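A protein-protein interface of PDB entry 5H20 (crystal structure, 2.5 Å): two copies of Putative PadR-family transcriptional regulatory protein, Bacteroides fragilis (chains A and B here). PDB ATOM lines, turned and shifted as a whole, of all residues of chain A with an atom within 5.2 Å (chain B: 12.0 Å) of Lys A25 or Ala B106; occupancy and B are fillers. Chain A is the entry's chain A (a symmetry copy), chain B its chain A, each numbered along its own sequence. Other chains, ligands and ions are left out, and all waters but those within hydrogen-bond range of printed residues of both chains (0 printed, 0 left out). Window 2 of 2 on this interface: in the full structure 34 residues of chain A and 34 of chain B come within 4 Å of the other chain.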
ATOM      1  N   LEU A  21      -8.642 -16.983 -15.090  1.00  0.00           N
ATOM      2  CA  LEU A  21      -9.509 -16.789 -16.259  1.00  0.00           C
ATOM      3  C   LEU A  21      -8.840 -17.193 -17.571  1.00  0.00           C
ATOM      4  O   LEU A  21      -9.398 -17.998 -18.317  1.00  0.00           O
ATOM      5  CB  LEU A  21     -10.018 -15.341 -16.366  1.00  0.00           C
ATOM      6  CG  LEU A  21     -11.512 -15.062 -16.216  1.00  0.00           C
ATOM      7  CD1 LEU A  21     -11.783 -13.620 -16.609  1.00  0.00           C
ATOM      8  CD2 LEU A  21     -12.373 -15.988 -17.070  1.00  0.00           C
ATOM      9  N   LEU A  22      -7.650 -16.646 -17.833  1.00  0.00           N
ATOM     10  CA  LEU A  22      -6.892 -16.934 -19.064  1.00  0.00           C
ATOM     11  C   LEU A  22      -6.445 -18.394 -19.185  1.00  0.00           C
ATOM     12  O   LEU A  22      -6.368 -18.923 -20.291  1.00  0.00           O
ATOM     13  CB  LEU A  22      -5.710 -15.964 -19.242  1.00  0.00           C
ATOM     14  CG  LEU A  22      -6.008 -14.473 -19.526  1.00  0.00           C
ATOM     15  CD1 LEU A  22      -4.811 -13.594 -19.187  1.00  0.00           C
ATOM     16  CD2 LEU A  22      -6.453 -14.216 -20.961  1.00  0.00           C
ATOM     17  N   LEU A  23      -6.199 -19.050 -18.052  1.00  0.00           N
ATOM     18  CA  LEU A  23      -5.753 -20.450 -18.044  1.00  0.00           C
ATOM     19  C   LEU A  23      -6.872 -21.499 -18.085  1.00  0.00           C
ATOM     20  O   LEU A  23      -6.606 -22.680 -18.317  1.00  0.00           O
ATOM     21  CB  LEU A  23      -4.797 -20.707 -16.869  1.00  0.00           C
ATOM     22  CG  LEU A  23      -3.374 -20.169 -17.048  1.00  0.00           C
ATOM     23  CD1 LEU A  23      -2.648 -20.201 -15.723  1.00  0.00           C
ATOM     24  CD2 LEU A  23      -2.555 -20.925 -18.097  1.00  0.00           C
ATOM     25  N   HIS A  24      -8.118 -21.055 -17.884  1.00  0.00           N
ATOM     26  CA  HIS A  24      -9.255 -21.964 -17.708  1.00  0.00           C
ATOM     27  C   HIS A  24      -9.582 -22.803 -18.941  1.00  0.00           C
ATOM     28  O   HIS A  24      -9.995 -23.954 -18.798  1.00  0.00           O
ATOM     29  CB  HIS A  24     -10.485 -21.228 -17.145  1.00  0.00           C
ATOM     30  CG  HIS A  24     -11.622 -21.066 -18.107  1.00  0.00           C
ATOM     31  ND1 HIS A  24     -12.623 -22.007 -18.243  1.00  0.00           N
ATOM     32  CD2 HIS A  24     -11.929 -20.064 -18.964  1.00  0.00           C
ATOM     33  CE1 HIS A  24     -13.490 -21.598 -19.153  1.00  0.00           C
ATOM     34  NE2 HIS A  24     -13.092 -20.423 -19.607  1.00  0.00           N
ATOM     35  N   LYS A  25      -9.393 -22.241 -20.134  1.00  0.00           N
ATOM     36  CA  LYS A  25      -9.627 -23.006 -21.360  1.00  0.00           C
ATOM     37  C   LYS A  25      -8.345 -23.633 -21.895  1.00  0.00           C
ATOM     38  O   LYS A  25      -8.335 -24.816 -22.247  1.00  0.00           O
ATOM     39  CB  LYS A  25     -10.325 -22.161 -22.426  1.00  0.00           C
ATOM     40  CG  LYS A  25     -11.324 -22.944 -23.263  1.00  0.00           C
ATOM     41  CD  LYS A  25     -12.439 -22.036 -23.750  1.00  0.00           C
ATOM     42  CE  LYS A  25     -13.572 -22.815 -24.394  1.00  0.00           C
ATOM     43  NZ  LYS A  25     -14.686 -21.906 -24.783  1.00  0.00           N
ATOM     44  N   GLU A  26      -7.272 -22.843 -21.939  1.00  0.00           N
ATOM     45  CA  GLU A  26      -6.000 -23.297 -22.479  1.00  0.00           C
ATOM     46  C   GLU A  26      -4.879 -23.247 -21.443  1.00  0.00           C
ATOM     47  O   GLU A  26      -4.723 -22.226 -20.764  1.00  0.00           O
ATOM     48  CB  GLU A  26      -5.610 -22.468 -23.704  1.00  0.00           C
ATOM     49  CG  GLU A  26      -6.240 -22.927 -25.014  1.00  0.00           C
ATOM     50  CD  GLU A  26      -5.814 -22.086 -26.215  1.00  0.00           C
ATOM     51  OE1 GLU A  26      -4.968 -21.161 -26.059  1.00  0.00           O
ATOM     52  OE2 GLU A  26      -6.325 -22.357 -27.332  1.00  0.00           O
ATOM     53  N   PRO A  27      -4.090 -24.345 -21.327  1.00  0.00           N
ATOM     54  CA  PRO A  27      -2.816 -24.249 -20.613  1.00  0.00           C
ATOM     55  C   PRO A  27      -1.863 -23.329 -21.381  1.00  0.00           C
ATOM     56  O   PRO A  27      -2.048 -23.128 -22.585  1.00  0.00           O
ATOM     57  CB  PRO A  27      -2.302 -25.690 -20.605  1.00  0.00           C
ATOM     58  CG  PRO A  27      -2.963 -26.349 -21.778  1.00  0.00           C
ATOM     59  CD  PRO A  27      -4.323 -25.710 -21.851  1.00  0.00           C
ATOM     60  N   GLU B  97     -12.913  -4.359 -18.014  1.00  0.00           N
ATOM     61  CA  GLU B  97     -11.792  -4.831 -18.844  1.00  0.00           C
ATOM     62  C   GLU B  97     -11.673  -6.361 -18.831  1.00  0.00           C
ATOM     63  O   GLU B  97     -11.320  -6.979 -19.847  1.00  0.00           O
ATOM     64  CB  GLU B  97     -10.473  -4.193 -18.389  1.00  0.00           C
ATOM     65  CG  GLU B  97      -9.280  -4.457 -19.306  1.00  0.00           C
ATOM     66  CD  GLU B  97      -9.401  -3.760 -20.656  1.00  0.00           C
ATOM     67  OE1 GLU B  97      -9.205  -2.530 -20.718  1.00  0.00           O
ATOM     68  OE2 GLU B  97      -9.692  -4.446 -21.659  1.00  0.00           O
ATOM     69  N   LEU B  98     -12.003  -6.953 -17.682  1.00  0.00           N
ATOM     70  CA  LEU B  98     -11.991  -8.400 -17.474  1.00  0.00           C
ATOM     71  C   LEU B  98     -13.070  -9.147 -18.284  1.00  0.00           C
ATOM     72  O   LEU B  98     -13.204 -10.373 -18.171  1.00  0.00           O
ATOM     73  CB  LEU B  98     -12.107  -8.691 -15.973  1.00  0.00           C
ATOM     74  CG  LEU B  98     -11.294  -9.767 -15.243  1.00  0.00           C
ATOM     75  CD1 LEU B  98     -10.088 -10.304 -16.004  1.00  0.00           C
ATOM     76  CD2 LEU B  98     -10.868  -9.198 -13.900  1.00  0.00           C
ATOM     77  N   ASN B  99     -13.824  -8.402 -19.098  1.00  0.00           N
ATOM     78  CA  ASN B  99     -14.740  -8.967 -20.093  1.00  0.00           C
ATOM     79  C   ASN B  99     -14.251  -8.846 -21.546  1.00  0.00           C
ATOM     80  O   ASN B  99     -14.769  -9.520 -22.444  1.00  0.00           O
ATOM     81  CB  ASN B  99     -16.152  -8.405 -19.923  1.00  0.00           C
ATOM     82  CG  ASN B  99     -16.863  -8.989 -18.720  1.00  0.00           C
ATOM     83  OD1 ASN B  99     -17.633  -9.939 -18.844  1.00  0.00           O
ATOM     84  ND2 ASN B  99     -16.598  -8.432 -17.542  1.00  0.00           N
ATOM     85  N   GLU B 100     -13.257  -7.982 -21.763  1.00  0.00           N
ATOM     86  CA  GLU B 100     -12.441  -8.010 -22.980  1.00  0.00           C
ATOM     87  C   GLU B 100     -11.421  -9.144 -22.862  1.00  0.00           C
ATOM     88  O   GLU B 100     -10.922  -9.651 -23.869  1.00  0.00           O
ATOM     89  CB  GLU B 100     -11.738  -6.668 -23.212  1.00  0.00           C
ATOM     90  CG  GLU B 100     -12.658  -5.516 -23.602  1.00  0.00           C
ATOM     91  CD  GLU B 100     -12.985  -5.481 -25.086  1.00  0.00           C
ATOM     92  OE1 GLU B 100     -13.734  -6.358 -25.567  1.00  0.00           O
ATOM     93  OE2 GLU B 100     -12.504  -4.555 -25.773  1.00  0.00           O
ATOM     94  N   THR B 101     -11.125  -9.522 -21.617  1.00  0.00           N
ATOM     95  CA  THR B 101     -10.355 -10.720 -21.285  1.00  0.00           C
ATOM     96  C   THR B 101     -11.210 -11.980 -21.504  1.00  0.00           C
ATOM     97  O   THR B 101     -10.722 -12.957 -22.076  1.00  0.00           O
ATOM     98  CB  THR B 101      -9.824 -10.656 -19.830  1.00  0.00           C
ATOM     99  OG1 THR B 101      -9.137  -9.415 -19.624  1.00  0.00           O
ATOM    100  CG2 THR B 101      -8.866 -11.803 -19.524  1.00  0.00           C
ATOM    101  N   VAL B 102     -12.479 -11.937 -21.081  1.00  0.00           N
ATOM    102  CA  VAL B 102     -13.415 -13.075 -21.204  1.00  0.00           C
ATOM    103  C   VAL B 102     -13.724 -13.464 -22.664  1.00  0.00           C
ATOM    104  O   VAL B 102     -14.258 -14.547 -22.933  1.00  0.00           O
ATOM    105  CB  VAL B 102     -14.701 -12.895 -20.337  1.00  0.00           C
ATOM    106  CG1 VAL B 102     -15.877 -12.340 -21.138  1.00  0.00           C
ATOM    107  CG2 VAL B 102     -15.097 -14.211 -19.681  1.00  0.00           C
ATOM    108  N   ASN B 103     -13.366 -12.577 -23.590  1.00  0.00           N
ATOM    109  CA  ASN B 103     -13.409 -12.871 -25.016  1.00  0.00           C
ATOM    110  C   ASN B 103     -12.198 -13.694 -25.468  1.00  0.00           C
ATOM    111  O   ASN B 103     -12.344 -14.605 -26.287  1.00  0.00           O
ATOM    112  CB  ASN B 103     -13.513 -11.580 -25.831  1.00  0.00           C
ATOM    113  CG  ASN B 103     -14.076 -11.812 -27.219  1.00  0.00           C
ATOM    114  OD1 ASN B 103     -15.270 -12.066 -27.385  1.00  0.00           O
ATOM    115  ND2 ASN B 103     -13.219 -11.714 -28.227  1.00  0.00           N
ATOM    116  N   HIS B 104     -11.018 -13.370 -24.930  1.00  0.00           N
ATOM    117  CA  HIS B 104      -9.773 -14.085 -25.254  1.00  0.00           C
ATOM    118  C   HIS B 104      -9.673 -15.462 -24.603  1.00  0.00           C
ATOM    119  O   HIS B 104      -8.990 -16.349 -25.128  1.00  0.00           O
ATOM    120  CB  HIS B 104      -8.539 -13.251 -24.891  1.00  0.00           C
ATOM    121  CG  HIS B 104      -8.405 -11.985 -25.681  1.00  0.00           C
ATOM    122  ND1 HIS B 104      -8.174 -10.764 -25.087  1.00  0.00           N
ATOM    123  CD2 HIS B 104      -8.477 -11.750 -27.013  1.00  0.00           C
ATOM    124  CE1 HIS B 104      -8.105  -9.830 -26.020  1.00  0.00           C
ATOM    125  NE2 HIS B 104      -8.287 -10.402 -27.196  1.00  0.00           N
ATOM    126  N   ILE B 105     -10.349 -15.629 -23.466  1.00  0.00           N
ATOM    127  CA  ILE B 105     -10.369 -16.904 -22.731  1.00  0.00           C
ATOM    128  C   ILE B 105     -11.182 -17.973 -23.472  1.00  0.00           C
ATOM    129  O   ILE B 105     -10.778 -19.136 -23.525  1.00  0.00           O
ATOM    130  CB  ILE B 105     -10.810 -16.743 -21.241  1.00  0.00           C
ATOM    131  CG1 ILE B 105     -12.269 -16.294 -21.084  1.00  0.00           C
ATOM    132  CG2 ILE B 105      -9.950 -15.704 -20.541  1.00  0.00           C
ATOM    133  CD1 ILE B 105     -13.289 -17.379 -20.808  1.00  0.00           C
ATOM    134  N   ALA B 106     -12.300 -17.552 -24.066  1.00  0.00           N
ATOM    135  CA  ALA B 106     -13.236 -18.443 -24.747  1.00  0.00           C
ATOM    136  C   ALA B 106     -12.866 -18.627 -26.216  1.00  0.00           C
ATOM    137  O   ALA B 106     -11.813 -19.177 -26.535  1.00  0.00           O
ATOM    138  CB  ALA B 106     -14.656 -17.914 -24.611  1.00  0.00           C
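The side-chain hydroxyl (OG1) of Thr B101 is in hydrogen-bond range of the backbone carbonyl oxygen (O) of Glu B97.
Leu A21 touches Leu B98. Ile B105 touches Leu A21 (CG2 to O, 3.2 Å). Leu A22 touches Thr B101. CA of Leu A22 touches CG2 of Ile B105 (3.6 Å). Ile B105 touches His A24. Ile B105 touches Lys A25. Lys A25 touches Ala B106 (NZ to CA, 3.8 Å).
Of the printed residues of chain B, Leu A21 touches Leu B98 (3.8 Å) and Ile B105 (3.2 Å). Of the printed residues of chain B, His A24 touches Ile B105. Lys A25 touches just these residues of chain B: Ile B105 (3.3 Å) and Ala B106 (3.8 Å). No residue of chain B comes within 4 Å of Glu A26. No residue of chain B comes within 4 Å of Pro A27. Of the printed residues of chain A, Leu B98 touches Leu A21 (3.8 Å). Of the printed residues of chain A, Thr B101 touches Leu A22 (3.7 Å). Val B102 touches none of the printed residues of chain A. Printed residues of chain A within 4 Å of Ile B105: Leu A21, Leu A22, His A24 and Lys A25. The nearest residue of chain B that does not touch Lys A25 is His B104 (6.5 Å).
Of the 7 printed residues of chain A, 4 touch a printed residue of chain B. Hydrophobic or aromatic side chains of chain A within 4 Å of the printed part of chain B: Leu A21, Leu A22 and His A24. Hydrophobic or aromatic side chains of chain B that line the printed part of chain A: Leu B98, Ile B105 and Ala B106. Among the printed residues, 7 pairs touch across the chains.
No position is printed for both chains. Of the 7 pairs that touch across the chains among the printed residues, none has its exchanged pair printed and touching as well.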
